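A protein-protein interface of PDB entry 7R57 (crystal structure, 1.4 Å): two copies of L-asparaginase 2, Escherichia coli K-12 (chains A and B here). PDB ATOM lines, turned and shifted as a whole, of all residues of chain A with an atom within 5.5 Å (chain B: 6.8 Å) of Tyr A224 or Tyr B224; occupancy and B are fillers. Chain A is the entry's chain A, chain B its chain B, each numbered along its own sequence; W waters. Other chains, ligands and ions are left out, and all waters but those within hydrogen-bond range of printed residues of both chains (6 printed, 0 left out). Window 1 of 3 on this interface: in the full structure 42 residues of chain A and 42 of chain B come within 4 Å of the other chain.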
ATOM      1  N   ILE A 222     -22.451 -34.591  -8.228  1.00  0.00           N
ATOM      2  CA  ILE A 222     -22.071 -33.525  -9.162  1.00  0.00           C
ATOM      3  C   ILE A 222     -20.627 -33.727  -9.590  1.00  0.00           C
ATOM      4  O   ILE A 222     -19.749 -33.899  -8.736  1.00  0.00           O
ATOM      5  CB  ILE A 222     -22.256 -32.129  -8.519  1.00  0.00           C
ATOM      6  CG1 ILE A 222     -23.711 -31.906  -8.089  1.00  0.00           C
ATOM      7  CG2 ILE A 222     -21.823 -31.054  -9.497  1.00  0.00           C
ATOM      8  CD1 ILE A 222     -23.992 -30.604  -7.373  1.00  0.00           C
ATOM      9  N   VAL A 223     -20.383 -33.669 -10.894  1.00  0.00           N
ATOM     10  CA  VAL A 223     -19.035 -33.718 -11.458  1.00  0.00           C
ATOM     11  C   VAL A 223     -18.726 -32.414 -12.200  1.00  0.00           C
ATOM     12  O   VAL A 223     -19.594 -31.844 -12.883  1.00  0.00           O
ATOM     13  CB  VAL A 223     -18.827 -34.955 -12.362  1.00  0.00           C
ATOM     14  CG1 VAL A 223     -18.954 -36.257 -11.555  1.00  0.00           C
ATOM     15  CG2 VAL A 223     -19.755 -34.969 -13.520  1.00  0.00           C
ATOM     16  N   TYR A 224     -17.495 -31.956 -12.087  1.00  0.00           N
ATOM     17  CA  TYR A 224     -17.047 -30.733 -12.726  1.00  0.00           C
ATOM     18  C   TYR A 224     -16.367 -31.014 -14.061  1.00  0.00           C
ATOM     19  O   TYR A 224     -15.684 -32.029 -14.238  1.00  0.00           O
ATOM     20  CB  TYR A 224     -16.048 -30.051 -11.790  1.00  0.00           C
ATOM     21  CG  TYR A 224     -15.968 -28.533 -11.889  1.00  0.00           C
ATOM     22  CD1 TYR A 224     -17.004 -27.749 -11.415  1.00  0.00           C
ATOM     23  CD2 TYR A 224     -14.852 -27.867 -12.425  1.00  0.00           C
ATOM     24  CE1 TYR A 224     -16.957 -26.369 -11.467  1.00  0.00           C
ATOM     25  CE2 TYR A 224     -14.801 -26.467 -12.474  1.00  0.00           C
ATOM     26  CZ  TYR A 224     -15.855 -25.741 -11.972  1.00  0.00           C
ATOM     27  OH  TYR A 224     -15.830 -24.369 -12.006  1.00  0.00           O
ATOM     28  N   ASN A 225     -16.529 -30.093 -15.000  1.00  0.00           N
ATOM     29  CA  ASN A 225     -15.841 -30.148 -16.281  1.00  0.00           C
ATOM     30  C   ASN A 225     -14.875 -28.975 -16.408  1.00  0.00           C
ATOM     31  O   ASN A 225     -15.125 -27.865 -15.897  1.00  0.00           O
ATOM     32  CB  ASN A 225     -16.792 -30.130 -17.474  1.00  0.00           C
ATOM     33  CG  ASN A 225     -17.637 -31.392 -17.590  1.00  0.00           C
ATOM     34  OD1 ASN A 225     -17.364 -32.266 -18.418  1.00  0.00           O
ATOM     35  ND2 ASN A 225     -18.703 -31.460 -16.804  1.00  0.00           N
ATOM     36  N   TYR A 226     -13.783 -29.232 -17.138  1.00  0.00           N
ATOM     37  CA  TYR A 226     -12.635 -28.360 -17.268  1.00  0.00           C
ATOM     38  C   TYR A 226     -11.727 -29.040 -18.287  1.00  0.00           C
ATOM     39  O   TYR A 226     -12.010 -30.148 -18.765  1.00  0.00           O
ATOM     40  CB  TYR A 226     -11.946 -28.124 -15.939  1.00  0.00           C
ATOM     41  CG  TYR A 226     -11.621 -29.388 -15.198  1.00  0.00           C
ATOM     42  CD1 TYR A 226     -12.584 -30.047 -14.456  1.00  0.00           C
ATOM     43  CD2 TYR A 226     -10.360 -29.943 -15.258  1.00  0.00           C
ATOM     44  CE1 TYR A 226     -12.312 -31.241 -13.773  1.00  0.00           C
ATOM     45  CE2 TYR A 226     -10.062 -31.118 -14.558  1.00  0.00           C
ATOM     46  CZ  TYR A 226     -11.023 -31.760 -13.826  1.00  0.00           C
ATOM     47  OH  TYR A 226     -10.673 -32.932 -13.149  1.00  0.00           O
ATOM     48  N   ALA A 229     -10.364 -32.949 -18.226  1.00  0.00           N
ATOM     49  CA  ALA A 229     -11.051 -33.503 -17.065  1.00  0.00           C
ATOM     50  C   ALA A 229     -10.980 -35.025 -17.011  1.00  0.00           C
ATOM     51  O   ALA A 229     -11.297 -35.707 -17.986  1.00  0.00           O
ATOM     52  CB  ALA A 229     -12.522 -33.073 -17.066  1.00  0.00           C
ATOM     53  N   ALA A 248     -21.550 -30.293 -14.010  1.00  0.00           N
ATOM     54  CA  ALA A 248     -21.228 -28.869 -14.027  1.00  0.00           C
ATOM     55  C   ALA A 248     -20.425 -28.663 -15.308  1.00  0.00           C
ATOM     56  O   ALA A 248     -19.200 -28.814 -15.320  1.00  0.00           O
ATOM     57  CB  ALA A 248     -20.485 -28.442 -12.776  1.00  0.00           C
ATOM     58  N   VAL A 259     -15.744 -37.452 -19.937  1.00  0.00           N
ATOM     59  CA  VAL A 259     -16.891 -37.345 -19.036  1.00  0.00           C
ATOM     60  C   VAL A 259     -18.178 -37.616 -19.789  1.00  0.00           C
ATOM     61  O   VAL A 259     -19.031 -38.391 -19.332  1.00  0.00           O
ATOM     62  CB  VAL A 259     -16.896 -35.956 -18.370  1.00  0.00           C
ATOM     63  CG1 VAL A 259     -18.073 -35.818 -17.441  1.00  0.00           C
ATOM     64  CG2 VAL A 259     -15.630 -35.690 -17.622  1.00  0.00           C
ATOM     65  N   ARG A 278     -21.012 -24.905 -14.970  1.00  0.00           N
ATOM     66  CA  ARG A 278     -20.219 -24.149 -14.014  1.00  0.00           C
ATOM     67  C   ARG A 278     -20.309 -22.638 -14.228  1.00  0.00           C
ATOM     68  O   ARG A 278     -19.816 -21.887 -13.378  1.00  0.00           O
ATOM     69  CB  ARG A 278     -18.755 -24.591 -14.114  1.00  0.00           C
ATOM     70  CG  ARG A 278     -18.063 -24.056 -15.359  1.00  0.00           C
ATOM     71  CD  ARG A 278     -16.628 -24.565 -15.482  1.00  0.00           C
ATOM     72  NE  ARG A 278     -15.902 -23.834 -16.522  1.00  0.00           N
ATOM     73  CZ  ARG A 278     -14.656 -24.104 -16.899  1.00  0.00           C
ATOM     74  NH1 ARG A 278     -14.022 -25.186 -16.465  1.00  0.00           N
ATOM     75  NH2 ARG A 278     -14.044 -23.305 -17.769  1.00  0.00           N
ATOM     76  N   PRO A 305     -25.439 -26.129 -10.763  1.00  0.00           N
ATOM     77  CA  PRO A 305     -25.305 -27.579 -10.524  1.00  0.00           C
ATOM     78  C   PRO A 305     -25.942 -28.034  -9.216  1.00  0.00           C
ATOM     79  O   PRO A 305     -26.636 -29.056  -9.177  1.00  0.00           O
ATOM     80  CB  PRO A 305     -23.793 -27.771 -10.583  1.00  0.00           C
ATOM     81  CG  PRO A 305     -23.302 -26.671 -11.535  1.00  0.00           C
ATOM     82  CD  PRO A 305     -24.187 -25.497 -11.228  1.00  0.00           C
ATOM     83  N   GLN A 306     -25.718 -27.278  -8.133  1.00  0.00           N
ATOM     84  CA  GLN A 306     -26.206 -27.647  -6.825  1.00  0.00           C
ATOM     85  C   GLN A 306     -27.720 -27.520  -6.757  1.00  0.00           C
ATOM     86  O   GLN A 306     -28.371 -28.307  -6.057  1.00  0.00           O
ATOM     87  CB  GLN A 306     -25.490 -26.852  -5.739  1.00  0.00           C
ATOM     88  CG  GLN A 306     -25.551 -25.324  -5.829  1.00  0.00           C
ATOM     89  CD  GLN A 306     -24.430 -24.719  -6.613  1.00  0.00           C
ATOM     90  OE1 GLN A 306     -23.787 -25.397  -7.398  1.00  0.00           O
ATOM     91  NE2 GLN A 306     -24.169 -23.449  -6.391  1.00  0.00           N
ATOM     92  N   GLU B 100      -9.233 -20.856 -19.284  1.00  0.00           N
ATOM     93  CA  GLU B 100      -8.197 -21.761 -18.783  1.00  0.00           C
ATOM     94  C   GLU B 100      -6.945 -21.656 -19.643  1.00  0.00           C
ATOM     95  O   GLU B 100      -5.847 -21.438 -19.124  1.00  0.00           O
ATOM     96  CB  GLU B 100      -8.743 -23.195 -18.760  1.00  0.00           C
ATOM     97  CG  GLU B 100      -9.984 -23.367 -17.870  1.00  0.00           C
ATOM     98  CD  GLU B 100     -10.579 -24.753 -17.930  1.00  0.00           C
ATOM     99  OE1 GLU B 100      -9.808 -25.719 -17.756  1.00  0.00           O
ATOM    100  OE2 GLU B 100     -11.788 -24.888 -18.146  1.00  0.00           O
ATOM    101  N   ILE B 222     -10.444 -31.757 -10.266  1.00  0.00           N
ATOM    102  CA  ILE B 222     -11.303 -30.820  -9.539  1.00  0.00           C
ATOM    103  C   ILE B 222     -12.511 -31.582  -9.006  1.00  0.00           C
ATOM    104  O   ILE B 222     -13.164 -32.308  -9.755  1.00  0.00           O
ATOM    105  CB  ILE B 222     -11.785 -29.651 -10.431  1.00  0.00           C
ATOM    106  CG1 ILE B 222     -10.587 -28.930 -11.050  1.00  0.00           C
ATOM    107  CG2 ILE B 222     -12.679 -28.715  -9.625  1.00  0.00           C
ATOM    108  CD1 ILE B 222     -10.936 -27.752 -11.975  1.00  0.00           C
ATOM    109  N   VAL B 223     -12.820 -31.361  -7.731  1.00  0.00           N
ATOM    110  CA  VAL B 223     -14.007 -31.917  -7.086  1.00  0.00           C
ATOM    111  C   VAL B 223     -14.930 -30.793  -6.614  1.00  0.00           C
ATOM    112  O   VAL B 223     -14.479 -29.772  -6.094  1.00  0.00           O
ATOM    113  CB  VAL B 223     -13.618 -32.862  -5.925  1.00  0.00           C
ATOM    114  CG1 VAL B 223     -12.827 -34.079  -6.457  1.00  0.00           C
ATOM    115  CG2 VAL B 223     -12.903 -32.169  -4.790  1.00  0.00           C
ATOM    116  N   TYR B 224     -16.237 -31.029  -6.712  1.00  0.00           N
ATOM    117  CA  TYR B 224     -17.232 -30.050  -6.329  1.00  0.00           C
ATOM    118  C   TYR B 224     -17.753 -30.331  -4.929  1.00  0.00           C
ATOM    119  O   TYR B 224     -17.855 -31.487  -4.506  1.00  0.00           O
ATOM    120  CB  TYR B 224     -18.393 -30.136  -7.315  1.00  0.00           C
ATOM    121  CG  TYR B 224     -19.169 -28.837  -7.532  1.00  0.00           C
ATOM    122  CD1 TYR B 224     -18.601 -27.792  -8.220  1.00  0.00           C
ATOM    123  CD2 TYR B 224     -20.497 -28.696  -7.120  1.00  0.00           C
ATOM    124  CE1 TYR B 224     -19.294 -26.602  -8.456  1.00  0.00           C
ATOM    125  CE2 TYR B 224     -21.212 -27.496  -7.359  1.00  0.00           C
ATOM    126  CZ  TYR B 224     -20.595 -26.484  -8.061  1.00  0.00           C
ATOM    127  OH  TYR B 224     -21.258 -25.305  -8.304  1.00  0.00           O
ATOM    128  N   ASN B 225     -18.108 -29.268  -4.214  1.00  0.00           N
ATOM    129  CA  ASN B 225     -18.733 -29.359  -2.909  1.00  0.00           C
ATOM    130  C   ASN B 225     -20.153 -28.809  -2.974  1.00  0.00           C
ATOM    131  O   ASN B 225     -20.445 -27.850  -3.717  1.00  0.00           O
ATOM    132  CB  ASN B 225     -17.960 -28.611  -1.829  1.00  0.00           C
ATOM    133  CG  ASN B 225     -16.646 -29.275  -1.485  1.00  0.00           C
ATOM    134  OD1 ASN B 225     -16.555 -30.016  -0.489  1.00  0.00           O
ATOM    135  ND2 ASN B 225     -15.622 -29.003  -2.270  1.00  0.00           N
ATOM    136  N   TYR B 226     -21.019 -29.423  -2.176  1.00  0.00           N
ATOM    137  CA  TYR B 226     -22.449 -29.154  -2.144  1.00  0.00           C
ATOM    138  C   TYR B 226     -22.994 -29.942  -0.956  1.00  0.00           C
ATOM    139  O   TYR B 226     -22.260 -30.699  -0.304  1.00  0.00           O
ATOM    140  CB  TYR B 226     -23.092 -29.538  -3.470  1.00  0.00           C
ATOM    141  CG  TYR B 226     -22.757 -30.954  -3.917  1.00  0.00           C
ATOM    142  CD1 TYR B 226     -21.543 -31.233  -4.565  1.00  0.00           C
ATOM    143  CD2 TYR B 226     -23.623 -32.004  -3.669  1.00  0.00           C
ATOM    144  CE1 TYR B 226     -21.224 -32.515  -4.962  1.00  0.00           C
ATOM    145  CE2 TYR B 226     -23.306 -33.282  -4.082  1.00  0.00           C
ATOM    146  CZ  TYR B 226     -22.118 -33.524  -4.739  1.00  0.00           C
ATOM    147  OH  TYR B 226     -21.794 -34.815  -5.142  1.00  0.00           O
ATOM    148  N   ALA B 229     -22.384 -34.017  -0.150  1.00  0.00           N
ATOM    149  CA  ALA B 229     -21.476 -34.378  -1.225  1.00  0.00           C
ATOM    150  C   ALA B 229     -20.768 -35.707  -0.976  1.00  0.00           C
ATOM    151  O   ALA B 229     -20.197 -35.936   0.095  1.00  0.00           O
ATOM    152  CB  ALA B 229     -20.431 -33.272  -1.381  1.00  0.00           C
ATOM    153  N   SER B 230     -20.739 -36.541  -2.004  1.00  0.00           N
ATOM    154  CA  SER B 230     -20.033 -37.809  -1.910  1.00  0.00           C
ATOM    155  C   SER B 230     -18.530 -37.571  -1.870  1.00  0.00           C
ATOM    156  O   SER B 230     -18.002 -36.687  -2.551  1.00  0.00           O
ATOM    157  CB  SER B 230     -20.312 -38.613  -3.155  1.00  0.00           C
ATOM    158  OG  SER B 230     -19.600 -39.845  -3.127  1.00  0.00           O
ATOM    159  N   PRO B 233     -15.717 -38.875  -5.671  1.00  0.00           N
ATOM    160  CA  PRO B 233     -14.853 -38.202  -6.660  1.00  0.00           C
ATOM    161  C   PRO B 233     -13.453 -37.928  -6.143  1.00  0.00           C
ATOM    162  O   PRO B 233     -12.457 -38.206  -6.839  1.00  0.00           O
ATOM    163  CB  PRO B 233     -15.650 -36.915  -6.935  1.00  0.00           C
ATOM    164  CG  PRO B 233     -17.068 -37.404  -6.845  1.00  0.00           C
ATOM    165  CD  PRO B 233     -17.061 -38.266  -5.615  1.00  0.00           C
ATOM    166  N   VAL B 246      -7.915 -29.858  -6.719  1.00  0.00           N
ATOM    167  CA  VAL B 246      -8.523 -28.562  -6.423  1.00  0.00           C
ATOM    168  C   VAL B 246      -9.944 -28.824  -5.957  1.00  0.00           C
ATOM    169  O   VAL B 246     -10.693 -29.540  -6.623  1.00  0.00           O
ATOM    170  CB  VAL B 246      -8.537 -27.684  -7.682  1.00  0.00           C
ATOM    171  CG1 VAL B 246      -9.346 -26.378  -7.465  1.00  0.00           C
ATOM    172  CG2 VAL B 246      -7.138 -27.331  -8.094  1.00  0.00           C
ATOM    173  N   SER B 247     -10.286 -28.261  -4.808  1.00  0.00           N
ATOM    174  CA  SER B 247     -11.655 -28.283  -4.303  1.00  0.00           C
ATOM    175  C   SER B 247     -12.421 -27.036  -4.738  1.00  0.00           C
ATOM    176  O   SER B 247     -12.028 -25.909  -4.417  1.00  0.00           O
ATOM    177  CB  SER B 247     -11.620 -28.353  -2.781  1.00  0.00           C
ATOM    178  OG  SER B 247     -12.918 -28.170  -2.238  1.00  0.00           O
ATOM    179  N   ALA B 248     -13.535 -27.244  -5.428  1.00  0.00           N
ATOM    180  CA  ALA B 248     -14.533 -26.182  -5.651  1.00  0.00           C
ATOM    181  C   ALA B 248     -15.397 -26.121  -4.402  1.00  0.00           C
ATOM    182  O   ALA B 248     -16.423 -26.806  -4.311  1.00  0.00           O
ATOM    183  CB  ALA B 248     -15.327 -26.420  -6.920  1.00  0.00           C
ATOM    184  N   GLY B 249     -14.924 -25.353  -3.416  1.00  0.00           N
ATOM    185  CA  GLY B 249     -15.563 -25.301  -2.115  1.00  0.00           C
ATOM    186  C   GLY B 249     -16.857 -24.516  -2.120  1.00  0.00           C
ATOM    187  O   GLY B 249     -17.235 -23.908  -3.114  1.00  0.00           O
ATOM    188  N   VAL B 250     -17.580 -24.576  -0.998  1.00  0.00           N
ATOM    189  CA  VAL B 250     -18.751 -23.725  -0.783  1.00  0.00           C
ATOM    190  C   VAL B 250     -18.296 -22.498  -0.014  1.00  0.00           C
ATOM    191  O   VAL B 250     -17.405 -22.563   0.826  1.00  0.00           O
ATOM    192  CB  VAL B 250     -19.869 -24.501  -0.060  1.00  0.00           C
ATOM    193  CG1 VAL B 250     -20.341 -25.619  -0.936  1.00  0.00           C
ATOM    194  CG2 VAL B 250     -19.424 -25.036   1.306  1.00  0.00           C
ATOM    195  N   TYR B 256     -17.418 -29.959   2.339  1.00  0.00           N
ATOM    196  CA  TYR B 256     -18.331 -30.908   2.983  1.00  0.00           C
ATOM    197  C   TYR B 256     -17.510 -31.926   3.775  1.00  0.00           C
ATOM    198  O   TYR B 256     -16.431 -32.334   3.331  1.00  0.00           O
ATOM    199  CB  TYR B 256     -19.177 -31.626   1.919  1.00  0.00           C
ATOM    200  CG  TYR B 256     -20.168 -32.571   2.528  1.00  0.00           C
ATOM    201  CD1 TYR B 256     -21.268 -32.082   3.191  1.00  0.00           C
ATOM    202  CD2 TYR B 256     -19.966 -33.952   2.498  1.00  0.00           C
ATOM    203  CE1 TYR B 256     -22.159 -32.924   3.808  1.00  0.00           C
ATOM    204  CE2 TYR B 256     -20.876 -34.795   3.094  1.00  0.00           C
ATOM    205  CZ  TYR B 256     -21.950 -34.272   3.766  1.00  0.00           C
ATOM    206  OH  TYR B 256     -22.858 -35.112   4.379  1.00  0.00           O
ATOM    207  N   VAL B 259     -15.720 -34.891   2.092  1.00  0.00           N
ATOM    208  CA  VAL B 259     -14.677 -34.447   1.180  1.00  0.00           C
ATOM    209  C   VAL B 259     -13.482 -33.930   1.962  1.00  0.00           C
ATOM    210  O   VAL B 259     -12.326 -34.246   1.641  1.00  0.00           O
ATOM    211  CB  VAL B 259     -15.246 -33.359   0.240  1.00  0.00           C
ATOM    212  CG1 VAL B 259     -14.193 -32.859  -0.718  1.00  0.00           C
ATOM    213  CG2 VAL B 259     -16.452 -33.903  -0.523  1.00  0.00           C
ATOM    214  N   SER B 277     -13.176 -22.100  -4.730  1.00  0.00           N
ATOM    215  CA  SER B 277     -14.595 -21.972  -4.432  1.00  0.00           C
ATOM    216  C   SER B 277     -15.452 -22.075  -5.678  1.00  0.00           C
ATOM    217  O   SER B 277     -15.105 -21.517  -6.721  1.00  0.00           O
ATOM    218  CB  SER B 277     -14.913 -20.632  -3.783  1.00  0.00           C
ATOM    219  OG  SER B 277     -16.295 -20.560  -3.479  1.00  0.00           O
ATOM    220  N   ARG B 278     -16.619 -22.720  -5.542  1.00  0.00           N
ATOM    221  CA  ARG B 278     -17.629 -22.670  -6.595  1.00  0.00           C
ATOM    222  C   ARG B 278     -18.283 -21.289  -6.738  1.00  0.00           C
ATOM    223  O   ARG B 278     -19.002 -21.057  -7.726  1.00  0.00           O
ATOM    224  CB  ARG B 278     -18.722 -23.702  -6.309  1.00  0.00           C
ATOM    225  CG  ARG B 278     -19.673 -23.292  -5.229  1.00  0.00           C
ATOM    226  CD  ARG B 278     -20.655 -24.395  -4.827  1.00  0.00           C
ATOM    227  NE  ARG B 278     -21.689 -23.904  -3.919  1.00  0.00           N
ATOM    228  CZ  ARG B 278     -22.698 -24.639  -3.475  1.00  0.00           C
ATOM    229  NH1 ARG B 278     -22.752 -25.938  -3.695  1.00  0.00           N
ATOM    230  NH2 ARG B 278     -23.674 -24.057  -2.791  1.00  0.00           N
ATOM    231  N   VAL B 279     -18.124 -20.435  -5.746  1.00  0.00           N
ATOM    232  CA  VAL B 279     -18.689 -19.080  -5.783  1.00  0.00           C
ATOM    233  C   VAL B 279     -17.950 -18.281  -6.849  1.00  0.00           C
ATOM    234  O   VAL B 279     -16.707 -18.321  -6.888  1.00  0.00           O
ATOM    235  CB  VAL B 279     -18.556 -18.467  -4.419  1.00  0.00           C
ATOM    236  CG1 VAL B 279     -19.071 -17.053  -4.393  1.00  0.00           C
ATOM    237  CG2 VAL B 279     -19.328 -19.298  -3.359  1.00  0.00           C
ATOM    238  N   ASN B 304     -10.526 -19.199  -9.532  1.00  0.00           N
ATOM    239  CA  ASN B 304     -11.649 -20.132  -9.506  1.00  0.00           C
ATOM    240  C   ASN B 304     -11.074 -21.538  -9.719  1.00  0.00           C
ATOM    241  O   ASN B 304      -9.877 -21.701  -9.963  1.00  0.00           O
ATOM    242  CB  ASN B 304     -12.730 -19.660 -10.492  1.00  0.00           C
ATOM    243  CG  ASN B 304     -12.313 -19.777 -11.938  1.00  0.00           C
ATOM    244  OD1 ASN B 304     -11.515 -20.642 -12.328  1.00  0.00           O
ATOM    245  ND2 ASN B 304     -12.904 -18.915 -12.790  1.00  0.00           N
ATOM    246  N   PRO B 305     -11.894 -22.575  -9.627  1.00  0.00           N
ATOM    247  CA  PRO B 305     -11.322 -23.936  -9.579  1.00  0.00           C
ATOM    248  C   PRO B 305     -10.498 -24.278 -10.801  1.00  0.00           C
ATOM    249  O   PRO B 305      -9.408 -24.851 -10.681  1.00  0.00           O
ATOM    250  CB  PRO B 305     -12.572 -24.807  -9.432  1.00  0.00           C
ATOM    251  CG  PRO B 305     -13.571 -23.906  -8.691  1.00  0.00           C
ATOM    252  CD  PRO B 305     -13.340 -22.558  -9.349  1.00  0.00           C
ATOM    253  N   GLN B 306     -11.003 -23.943 -11.991  1.00  0.00           N
ATOM    254  CA  GLN B 306     -10.312 -24.292 -13.216  1.00  0.00           C
ATOM    255  C   GLN B 306      -9.038 -23.477 -13.387  1.00  0.00           C
ATOM    256  O   GLN B 306      -8.056 -23.978 -13.941  1.00  0.00           O
ATOM    257  CB  GLN B 306     -11.224 -24.197 -14.425  1.00  0.00           C
ATOM    258  CG  GLN B 306     -11.913 -22.852 -14.653  1.00  0.00           C
ATOM    259  CD  GLN B 306     -13.242 -22.713 -13.952  1.00  0.00           C
ATOM    260  OE1 GLN B 306     -13.545 -23.430 -13.028  1.00  0.00           O
ATOM    261  NE2 GLN B 306     -14.067 -21.764 -14.419  1.00  0.00           N
HETATM  262  O   HOH W   1     -19.740 -20.336 -10.744  1.00  0.00           O
HETATM  263  O   HOH W   2     -16.826 -21.251 -13.295  1.00  0.00           O
HETATM  264  O   HOH W   3     -17.302 -23.036  -9.951  1.00  0.00           O
HETATM  265  O   HOH W   4     -17.114 -33.582  -7.991  1.00  0.00           O
HETATM  266  O   HOH W   5     -21.924 -21.942  -7.836  1.00  0.00           O
HETATM  267  O   HOH W   6     -15.566 -33.484 -10.318  1.00  0.00           O
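The guanidinium group of Arg A278 lies close to the side-chain amide nitrogen of Gln B306, at 3.5 Å.
The guanidinium group of Arg A278 lies within salt-bridge range of the side-chain carboxylate of Glu B100 (2.8 Å).
The backbone NH of Ile A222 sits at hydrogen-bond distance from the side-chain hydroxyl of Tyr B226 (3.2 Å).
N of Ile B222 sits at hydrogen-bond distance from OH of Tyr A226, at 3.1 Å.
The side-chain hydroxyl of Tyr A224 lies within hydrogen-bond range of the side-chain amide oxygen of Gln B306 (2.7 Å).
The side-chain amide oxygen of Gln A306 lies within hydrogen-bond range of the side-chain hydroxyl of Tyr B224 (2.7 Å).
O of Asn A225 lies within hydrogen-bond range of NH1 of Arg A278.
The backbone carbonyl oxygen of Gly B249 lies within hydrogen-bond range of the backbone NH of Arg B278, 2.8 Å away.
The backbone NH (N) of Gln B306 lies close to the side-chain amide oxygen (OD1) of Asn B304, 3.4 Å away.
The guanidinium group (NH1) of Arg B278 sits at hydrogen-bond distance from the backbone carbonyl oxygen (O) of Asn B225 (3.0 Å).
Tyr B224 touches Ile A222 (CD2 to CG2, 3.6 Å).
Ile B222 touches Tyr A224.
Tyr B224 touches Tyr A224 (CD1 to CD1, 3.6 Å).
Tyr A226 touches Glu B100 (CA to OE2, 3.7 Å).
Gln A306 touches Arg B278.
Of chain B, only Ile B222 (3.6 Å), Tyr B224 (3.6 Å) and Gln B306 (2.7 Å) come within 4 Å of Tyr A224.
Pro A305 touches none of the printed residues of chain B.
Printed residues of chain B within 4 Å of Gln A306: Tyr B224 (2.7 Å) and Arg B278 (3.5 Å).
Printed residues of chain A within 4 Å of Tyr B224: Ile A222 (3.6 Å), Tyr A224 (3.6 Å) and Gln A306 (2.7 Å).
Of the printed residues of chain A, Tyr B226 touches Ile A222.
Ala B248 touches none of the printed residues of chain A.
Of the printed residues of chain A, Arg B278 touches Gln A306.
Printed residues of chain A within 4 Å of Gln B306: Tyr A224 (2.7 Å) and Arg A278 (3.5 Å).
The nearest residue of chain B that does not touch Tyr A224 is Pro B305 (4.04 Å).
The nearest residue of chain A that does not touch Tyr B224 is Pro A305 (4.1 Å).
Hydrophobic or aromatic side chains of chain A within 4 Å of the printed part of chain B: Ile A222, Tyr A224 and Tyr A226.
Hydrophobic or aromatic side chains of chain B that line the printed part of chain A: Ile B222, Tyr B224 and Tyr B226.
Along chain B the printed residues that touch a printed residue of chain A span positions 100 to 306.
Among the printed residues, 11 pairs touch across the chains.
Ile A222 touches Tyr B224, and with the chains exchanged Tyr A224 touches Ile B222.
Ile A222 touches Tyr B226, and with the chains exchanged Tyr A226 touches Ile B222.
Tyr B224 touches its own counterpart, Tyr A224.
Arg A278 touches Gln B306, and with the chains exchanged Gln A306 touches Arg B278.
Positions printed for both chains: 222, 223, 224, 225, 226, 229, 248, 259, 278, 305 and 306.
Of the 11 pairs that touch across the chains among the printed residues, 9 have their exchanged pair printed and touching as well.
Water W6 bridges O of Ile B222 and N of Tyr A224.
Water W4 lies within hydrogen-bond range of O of Ile A222 (2.8 Å) and N of Tyr B224 (3.0 Å).
Water W3 bridges the side-chain hydroxyl (OH) of Tyr A224 and the backbone carbonyl oxygen (O) of Arg B278.
Water W2 bridges NE2 of Gln B306 (3.0 Å) and O of Arg A278 (3.1 Å).
Water W5 lies within hydrogen-bond range of O of Arg B278 (3.1 Å), NE2 of Gln A306 (3.1 Å) and OH of Tyr B224 (3.5 Å).
Water W1 lies within hydrogen-bond range of O of Arg A278 and O of Arg B278.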
